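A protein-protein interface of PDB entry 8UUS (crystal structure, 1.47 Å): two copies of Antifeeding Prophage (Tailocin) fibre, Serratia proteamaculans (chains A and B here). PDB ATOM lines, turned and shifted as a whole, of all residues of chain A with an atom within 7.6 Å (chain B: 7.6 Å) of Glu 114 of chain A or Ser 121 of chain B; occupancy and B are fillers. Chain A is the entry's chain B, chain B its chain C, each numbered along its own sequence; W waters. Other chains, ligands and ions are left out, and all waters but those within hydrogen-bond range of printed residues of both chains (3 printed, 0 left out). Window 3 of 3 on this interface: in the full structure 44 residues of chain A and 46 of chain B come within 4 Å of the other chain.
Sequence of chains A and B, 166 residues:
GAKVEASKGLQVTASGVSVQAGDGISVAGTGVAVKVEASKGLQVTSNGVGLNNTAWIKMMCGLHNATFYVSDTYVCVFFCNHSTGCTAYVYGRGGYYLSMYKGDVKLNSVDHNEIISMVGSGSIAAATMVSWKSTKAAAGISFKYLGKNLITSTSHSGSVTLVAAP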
ATOM      1  N   CYS A  86       7.681  -7.305 -24.247  1.00  0.00           N
ATOM      2  CA  CYS A  86       8.914  -6.632 -24.626  1.00  0.00           C
ATOM      3  C   CYS A  86      10.055  -7.264 -23.847  1.00  0.00           C
ATOM      4  O   CYS A  86       9.883  -7.661 -22.693  1.00  0.00           O
ATOM      5  CB  CYS A  86       8.792  -5.129 -24.301  1.00  0.00           C
ATOM      6  SG  CYS A  86      10.270  -4.115 -24.494  1.00  0.00           S
ATOM      7  N   THR A  87      11.227  -7.353 -24.483  1.00  0.00           N
ATOM      8  CA  THR A  87      12.465  -7.638 -23.764  1.00  0.00           C
ATOM      9  C   THR A  87      13.497  -6.578 -24.119  1.00  0.00           C
ATOM     10  O   THR A  87      13.597  -6.156 -25.276  1.00  0.00           O
ATOM     11  CB  THR A  87      13.005  -9.044 -24.082  1.00  0.00           C
ATOM     12  OG1 THR A  87      12.054 -10.025 -23.640  1.00  0.00           O
ATOM     13  CG2 THR A  87      14.337  -9.290 -23.375  1.00  0.00           C
ATOM     14  N   ALA A  88      14.246  -6.143 -23.113  1.00  0.00           N
ATOM     15  CA  ALA A  88      15.231  -5.088 -23.263  1.00  0.00           C
ATOM     16  C   ALA A  88      16.614  -5.568 -22.844  1.00  0.00           C
ATOM     17  O   ALA A  88      16.768  -6.378 -21.920  1.00  0.00           O
ATOM     18  CB  ALA A  88      14.839  -3.882 -22.419  1.00  0.00           C
ATOM     19  N   ASP A 111       5.536  -3.961 -13.353  1.00  0.00           N
ATOM     20  CA  ASP A 111       6.753  -4.608 -12.871  1.00  0.00           C
ATOM     21  C   ASP A 111       7.228  -5.677 -13.846  1.00  0.00           C
ATOM     22  O   ASP A 111       6.436  -6.352 -14.501  1.00  0.00           O
ATOM     23  CB  ASP A 111       6.533  -5.252 -11.502  1.00  0.00           C
ATOM     24  CG  ASP A 111       6.411  -4.233 -10.391  1.00  0.00           C
ATOM     25  OD1 ASP A 111       7.143  -3.219 -10.414  1.00  0.00           O
ATOM     26  OD2 ASP A 111       5.591  -4.466  -9.483  1.00  0.00           O
ATOM     27  N   HIS A 112       8.546  -5.833 -13.925  1.00  0.00           N
ATOM     28  CA  HIS A 112       9.138  -6.766 -14.869  1.00  0.00           C
ATOM     29  C   HIS A 112       8.817  -8.205 -14.497  1.00  0.00           C
ATOM     30  O   HIS A 112       8.453  -8.524 -13.360  1.00  0.00           O
ATOM     31  CB  HIS A 112      10.661  -6.615 -14.888  1.00  0.00           C
ATOM     32  CG  HIS A 112      11.317  -6.922 -13.578  1.00  0.00           C
ATOM     33  ND1 HIS A 112      11.574  -8.211 -13.150  1.00  0.00           N
ATOM     34  CD2 HIS A 112      11.784  -6.103 -12.606  1.00  0.00           C
ATOM     35  CE1 HIS A 112      12.160  -8.167 -11.966  1.00  0.00           C
ATOM     36  NE2 HIS A 112      12.303  -6.900 -11.618  1.00  0.00           N
ATOM     37  N   ASN A 113       8.983  -9.086 -15.483  1.00  0.00           N
ATOM     38  CA  ASN A 113       8.974 -10.523 -15.253  1.00  0.00           C
ATOM     39  C   ASN A 113      10.409 -11.046 -15.248  1.00  0.00           C
ATOM     40  O   ASN A 113      11.236 -10.569 -14.459  1.00  0.00           O
ATOM     41  CB  ASN A 113       8.059 -11.218 -16.265  1.00  0.00           C
ATOM     42  CG  ASN A 113       6.606 -10.750 -16.137  1.00  0.00           C
ATOM     43  OD1 ASN A 113       6.133  -9.900 -16.896  1.00  0.00           O
ATOM     44  ND2 ASN A 113       5.920 -11.264 -15.130  1.00  0.00           N
ATOM     45  N   GLU A 114      10.738 -12.002 -16.112  1.00  0.00           N
ATOM     46  CA  GLU A 114      12.036 -12.655 -16.009  1.00  0.00           C
ATOM     47  C   GLU A 114      13.160 -11.678 -16.320  1.00  0.00           C
ATOM     48  O   GLU A 114      13.041 -10.844 -17.220  1.00  0.00           O
ATOM     49  CB  GLU A 114      12.132 -13.823 -16.988  1.00  0.00           C
ATOM     50  CG  GLU A 114      11.169 -14.978 -16.704  1.00  0.00           C
ATOM     51  CD  GLU A 114      11.416 -15.676 -15.381  1.00  0.00           C
ATOM     52  OE1 GLU A 114      12.512 -15.543 -14.799  1.00  0.00           O
ATOM     53  OE2 GLU A 114      10.500 -16.389 -14.909  1.00  0.00           O
ATOM     54  N   ILE A 115      14.254 -11.794 -15.563  1.00  0.00           N
ATOM     55  CA  ILE A 115      15.488 -11.052 -15.807  1.00  0.00           C
ATOM     56  C   ILE A 115      16.632 -12.052 -15.909  1.00  0.00           C
ATOM     57  O   ILE A 115      16.681 -13.033 -15.160  1.00  0.00           O
ATOM     58  CB  ILE A 115      15.765 -10.040 -14.672  1.00  0.00           C
ATOM     59  CG1 ILE A 115      14.728  -8.915 -14.694  1.00  0.00           C
ATOM     60  CG2 ILE A 115      17.172  -9.461 -14.793  1.00  0.00           C
ATOM     61  CD1 ILE A 115      15.021  -7.778 -13.708  1.00  0.00           C
ATOM     62  N   ILE A 116      17.546 -11.813 -16.848  1.00  0.00           N
ATOM     63  CA  ILE A 116      18.835 -12.494 -16.903  1.00  0.00           C
ATOM     64  C   ILE A 116      19.904 -11.510 -16.437  1.00  0.00           C
ATOM     65  O   ILE A 116      19.854 -10.323 -16.780  1.00  0.00           O
ATOM     66  CB  ILE A 116      19.112 -12.991 -18.334  1.00  0.00           C
ATOM     67  CG1 ILE A 116      18.129 -14.099 -18.704  1.00  0.00           C
ATOM     68  CG2 ILE A 116      20.530 -13.487 -18.460  1.00  0.00           C
ATOM     69  CD1 ILE A 116      18.321 -14.625 -20.120  1.00  0.00           C
ATOM     70  N   SER A 117      20.847 -11.994 -15.632  1.00  0.00           N
ATOM     71  CA  SER A 117      21.773 -11.131 -14.912  1.00  0.00           C
ATOM     72  C   SER A 117      23.206 -11.641 -15.001  1.00  0.00           C
ATOM     73  O   SER A 117      23.459 -12.816 -15.280  1.00  0.00           O
ATOM     74  CB  SER A 117      21.422 -11.102 -13.417  1.00  0.00           C
ATOM     75  OG  SER A 117      20.141 -10.534 -13.204  1.00  0.00           O
ATOM     76  N   MET A 129      19.255  -8.555 -19.224  1.00  0.00           N
ATOM     77  CA  MET A 129      18.080  -8.636 -20.076  1.00  0.00           C
ATOM     78  C   MET A 129      16.883  -8.581 -19.144  1.00  0.00           C
ATOM     79  O   MET A 129      16.859  -9.290 -18.134  1.00  0.00           O
ATOM     80  CB  MET A 129      18.054  -9.937 -20.891  1.00  0.00           C
ATOM     81  CG  MET A 129      19.091  -9.975 -22.005  1.00  0.00           C
ATOM     82  SD  MET A 129      19.006 -11.539 -22.913  1.00  0.00           S
ATOM     83  CE  MET A 129      17.418 -11.344 -23.717  1.00  0.00           C
ATOM     84  N   VAL A 130      15.917  -7.725 -19.465  1.00  0.00           N
ATOM     85  CA  VAL A 130      14.726  -7.543 -18.638  1.00  0.00           C
ATOM     86  C   VAL A 130      13.505  -7.680 -19.535  1.00  0.00           C
ATOM     87  O   VAL A 130      13.445  -7.063 -20.605  1.00  0.00           O
ATOM     88  CB  VAL A 130      14.723  -6.176 -17.927  1.00  0.00           C
ATOM     89  CG1 VAL A 130      13.503  -6.067 -17.034  1.00  0.00           C
ATOM     90  CG2 VAL A 130      15.995  -5.979 -17.095  1.00  0.00           C
ATOM     91  N   SER A 131      12.530  -8.484 -19.105  1.00  0.00           N
ATOM     92  CA  SER A 131      11.339  -8.733 -19.902  1.00  0.00           C
ATOM     93  C   SER A 131      10.067  -8.336 -19.164  1.00  0.00           C
ATOM     94  O   SER A 131      10.013  -8.352 -17.927  1.00  0.00           O
ATOM     95  CB  SER A 131      11.248 -10.206 -20.323  1.00  0.00           C
ATOM     96  OG  SER A 131      11.043 -11.062 -19.207  1.00  0.00           O
ATOM     97  N   TRP A 132       9.060  -7.962 -19.954  1.00  0.00           N
ATOM     98  CA  TRP A 132       7.693  -7.721 -19.487  1.00  0.00           C
ATOM     99  C   TRP A 132       6.779  -8.534 -20.390  1.00  0.00           C
ATOM    100  O   TRP A 132       6.716  -8.285 -21.597  1.00  0.00           O
ATOM    101  CB  TRP A 132       7.328  -6.235 -19.576  1.00  0.00           C
ATOM    102  CG  TRP A 132       8.135  -5.347 -18.680  1.00  0.00           C
ATOM    103  CD1 TRP A 132       7.783  -4.873 -17.434  1.00  0.00           C
ATOM    104  CD2 TRP A 132       9.426  -4.802 -18.966  1.00  0.00           C
ATOM    105  NE1 TRP A 132       8.792  -4.088 -16.928  1.00  0.00           N
ATOM    106  CE2 TRP A 132       9.806  -4.015 -17.854  1.00  0.00           C
ATOM    107  CE3 TRP A 132      10.301  -4.898 -20.058  1.00  0.00           C
ATOM    108  CZ2 TRP A 132      11.027  -3.346 -17.802  1.00  0.00           C
ATOM    109  CZ3 TRP A 132      11.511  -4.224 -20.000  1.00  0.00           C
ATOM    110  CH2 TRP A 132      11.855  -3.452 -18.880  1.00  0.00           C
ATOM    111  N   LYS A 133       6.067  -9.501 -19.813  1.00  0.00           N
ATOM    112  CA  LYS A 133       5.358 -10.469 -20.642  1.00  0.00           C
ATOM    113  C   LYS A 133       4.221  -9.849 -21.448  1.00  0.00           C
ATOM    114  O   LYS A 133       3.877 -10.359 -22.524  1.00  0.00           O
ATOM    115  CB  LYS A 133       4.862 -11.645 -19.792  1.00  0.00           C
ATOM    116  CG  LYS A 133       5.966 -12.576 -19.293  1.00  0.00           C
ATOM    117  CD  LYS A 133       5.443 -13.585 -18.273  1.00  0.00           C
ATOM    118  CE  LYS A 133       6.489 -14.662 -17.988  1.00  0.00           C
ATOM    119  NZ  LYS A 133       5.983 -15.705 -17.041  1.00  0.00           N
ATOM    120  N   VAL B 119      22.880 -15.454 -16.349  1.00  0.00           N
ATOM    121  CA  VAL B 119      22.011 -16.428 -15.690  1.00  0.00           C
ATOM    122  C   VAL B 119      20.689 -15.795 -15.290  1.00  0.00           C
ATOM    123  O   VAL B 119      20.650 -14.664 -14.795  1.00  0.00           O
ATOM    124  CB  VAL B 119      22.687 -17.101 -14.480  1.00  0.00           C
ATOM    125  CG1 VAL B 119      23.820 -17.986 -14.962  1.00  0.00           C
ATOM    126  CG2 VAL B 119      23.183 -16.056 -13.500  1.00  0.00           C
ATOM    127  N   GLY B 120      19.603 -16.540 -15.534  1.00  0.00           N
ATOM    128  CA  GLY B 120      18.290 -16.198 -15.067  1.00  0.00           C
ATOM    129  C   GLY B 120      17.811 -17.136 -13.976  1.00  0.00           C
ATOM    130  O   GLY B 120      18.594 -17.832 -13.321  1.00  0.00           O
ATOM    131  N   SER B 121      16.505 -17.131 -13.765  1.00  0.00           N
ATOM    132  CA  SER B 121      15.927 -17.993 -12.750  1.00  0.00           C
ATOM    133  C   SER B 121      15.936 -19.441 -13.227  1.00  0.00           C
ATOM    134  O   SER B 121      15.862 -19.728 -14.426  1.00  0.00           O
ATOM    135  CB  SER B 121      14.495 -17.560 -12.447  1.00  0.00           C
ATOM    136  OG  SER B 121      13.683 -17.658 -13.598  1.00  0.00           O
ATOM    137  N   GLY B 122      16.034 -20.353 -12.273  1.00  0.00           N
ATOM    138  CA  GLY B 122      16.004 -21.769 -12.606  1.00  0.00           C
ATOM    139  C   GLY B 122      17.102 -22.131 -13.589  1.00  0.00           C
ATOM    140  O   GLY B 122      18.294 -21.889 -13.347  1.00  0.00           O
ATOM    141  N   SER B 123      16.715 -22.722 -14.718  1.00  0.00           N
ATOM    142  CA  SER B 123      17.677 -23.170 -15.716  1.00  0.00           C
ATOM    143  C   SER B 123      17.925 -22.139 -16.812  1.00  0.00           C
ATOM    144  O   SER B 123      18.708 -22.413 -17.731  1.00  0.00           O
ATOM    145  CB  SER B 123      17.211 -24.484 -16.345  1.00  0.00           C
ATOM    146  OG  SER B 123      16.010 -24.277 -17.059  1.00  0.00           O
ATOM    147  N   ILE B 124      17.287 -20.968 -16.737  1.00  0.00           N
ATOM    148  CA  ILE B 124      17.459 -19.958 -17.774  1.00  0.00           C
ATOM    149  C   ILE B 124      18.901 -19.483 -17.776  1.00  0.00           C
ATOM    150  O   ILE B 124      19.461 -19.116 -16.733  1.00  0.00           O
ATOM    151  CB  ILE B 124      16.495 -18.786 -17.551  1.00  0.00           C
ATOM    152  CG1 ILE B 124      15.043 -19.197 -17.807  1.00  0.00           C
ATOM    153  CG2 ILE B 124      16.834 -17.607 -18.469  1.00  0.00           C
ATOM    154  CD1 ILE B 124      14.070 -18.178 -17.281  1.00  0.00           C
ATOM    155  N   ALA B 125      19.508 -19.473 -18.958  1.00  0.00           N
ATOM    156  CA  ALA B 125      20.882 -19.019 -19.095  1.00  0.00           C
ATOM    157  C   ALA B 125      21.090 -18.628 -20.546  1.00  0.00           C
ATOM    158  O   ALA B 125      20.613 -19.318 -21.449  1.00  0.00           O
ATOM    159  CB  ALA B 125      21.878 -20.112 -18.700  1.00  0.00           C
ATOM    160  N   ASN B 149      13.559 -17.161 -25.690  1.00  0.00           N
ATOM    161  CA  ASN B 149      13.110 -15.865 -25.209  1.00  0.00           C
ATOM    162  C   ASN B 149      12.491 -16.041 -23.830  1.00  0.00           C
ATOM    163  O   ASN B 149      12.198 -17.158 -23.395  1.00  0.00           O
ATOM    164  CB  ASN B 149      12.161 -15.183 -26.213  1.00  0.00           C
ATOM    165  CG  ASN B 149      10.759 -15.735 -26.159  1.00  0.00           C
ATOM    166  OD1 ASN B 149       9.912 -15.203 -25.446  1.00  0.00           O
ATOM    167  ND2 ASN B 149      10.494 -16.792 -26.921  1.00  0.00           N
ATOM    168  N   LEU B 150      12.311 -14.915 -23.134  1.00  0.00           N
ATOM    169  CA  LEU B 150      11.872 -14.931 -21.743  1.00  0.00           C
ATOM    170  C   LEU B 150      10.363 -14.872 -21.583  1.00  0.00           C
ATOM    171  O   LEU B 150       9.871 -15.044 -20.461  1.00  0.00           O
ATOM    172  CB  LEU B 150      12.475 -13.737 -21.003  1.00  0.00           C
ATOM    173  CG  LEU B 150      13.992 -13.879 -20.874  1.00  0.00           C
ATOM    174  CD1 LEU B 150      14.603 -12.583 -20.336  1.00  0.00           C
ATOM    175  CD2 LEU B 150      14.398 -15.082 -20.022  1.00  0.00           C
ATOM    176  N   ILE B 151       9.629 -14.597 -22.655  1.00  0.00           N
ATOM    177  CA  ILE B 151       8.178 -14.474 -22.565  1.00  0.00           C
ATOM    178  C   ILE B 151       7.487 -15.810 -22.798  1.00  0.00           C
ATOM    179  O   ILE B 151       6.644 -16.231 -21.999  1.00  0.00           O
ATOM    180  CB  ILE B 151       7.687 -13.375 -23.524  1.00  0.00           C
ATOM    181  CG1 ILE B 151       8.284 -12.030 -23.085  1.00  0.00           C
ATOM    182  CG2 ILE B 151       6.155 -13.327 -23.543  1.00  0.00           C
ATOM    183  CD1 ILE B 151       7.851 -10.829 -23.925  1.00  0.00           C
HETATM  184  O   HOH W   1      15.207 -15.348 -15.534  1.00  0.00           O
HETATM  185  O   HOH W   2       9.385 -12.980 -18.607  1.00  0.00           O
HETATM  186  O   HOH W   3      13.178 -12.388 -24.028  1.00  0.00           O
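Of the 10 printed residues of chain B, 6 touch a printed residue of chain A. Hydrophobic or aromatic side chains of chain B that line the printed part of chain A: Val 119, Ile 124, Leu 150 and Ile 151. Printed residues of chain A that touch a printed residue of chain B: Cys 86, Glu 114, Ile 115, Ile 116, Ser 117, Ser 131, Trp 132 and Lys 133. Among the printed residues, no Asp or Glu carboxylate lies within 4 Å of a Lys or Arg side-chain nitrogen of the other chain.
Water W2 lies within hydrogen-bond range of the side-chain hydroxyl of Ser 131 of chain A (2.6 Å), the backbone carbonyl oxygen of Leu 150 of chain B (2.8 Å) and the backbone NH of Glu 114 of chain A (3.0 Å). Water W3 lies within hydrogen-bond range of the side-chain hydroxyl (OG1) of Thr 87 of chain A (2.6 Å) and the backbone NH (N) of Leu 150 of chain B (2.8 Å). Water W1 lies within hydrogen-bond range of the backbone carbonyl oxygen (O) of Ile 115 of chain A (2.8 Å), the side-chain carboxylate (OE1) of Glu 114 of chain A (2.8 Å) and the backbone NH (N) of Ser 121 of chain B (2.8 Å).
Printed residues of chain B within 4 Å of Ile 115 of chain A: Gly 120. Val 130 of chain A touches none of the printed residues of chain B. Of the printed residues of chain B, Trp 132 of chain A touches Ile 151. Of the printed residues of chain A, Ser 121 of chain B touches Glu 114. Of the printed residues of chain A, Leu 150 of chain B touches Glu 114, Ile 116 and Ser 131. The nearest residue of chain B that does not touch Glu 114 of chain A is Gly 120 of chain B (5.6 Å). The nearest printed residue of chain B that does not touch Trp 132 of chain A is Leu 150 of chain B (6.8 Å).
The side-chain hydroxyl of Ser 131 of chain A lies within hydrogen-bond range of the backbone carbonyl oxygen of Glu 114 of chain A, 2.8 Å away. The backbone carbonyl oxygen (O) of Ser 131 of chain A sits at hydrogen-bond distance from the backbone NH (N) of Asn 113 of chain A, 2.8 Å away. O of Cys 86 of chain A sits at hydrogen-bond distance from N of Trp 132 of chain A, 2.9 Å away. OD1 of Asn 113 of chain A lies within hydrogen-bond range of N of Lys 133 of chain A (2.9 Å). OD1 of Asn 149 of chain B sits at hydrogen-bond distance from N of Ile 151 of chain B (2.9 Å). O of Met 129 of chain A lies within hydrogen-bond range of N of Ile 116 of chain A, 2.9 Å away.
N of Cys 86 of chain A touches CD1 of Ile 151 of chain B (3.5 Å). CD1 of Ile 124 of chain B touches OE1 of Glu 114 of chain A, 3.9 Å away. Glu 114 of chain A touches Leu 150 of chain B. Gly 120 of chain B touches Ile 115 of chain A. Ile 116 of chain A touches Val 119 of chain B (CA to O, 3.5 Å). Ile 124 of chain B touches Ile 116 of chain A. Ile 116 of chain A touches Leu 150 of chain B (CD1 to CD2, 3.95 Å). Ser 131 of chain A touches Leu 150 of chain B. O of Trp 132 of chain A touches CD1 of Ile 151 of chain B, at 3.6 Å. Lys 133 of chain A touches Ile 151 of chain B.
The backbone NH (N) of Ser 117 of chain A sits at hydrogen-bond distance from the backbone carbonyl oxygen (O) of Val 119 of chain B. The side-chain carboxylate of Glu 114 of chain A is in hydrogen-bond range of the side-chain hydroxyl of Ser 121 of chain B, 2.7 Å away.
No position is printed for both chains. Of the 12 pairs that touch across the chains among the printed residues, none has its exchanged pair printed and touching as well.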
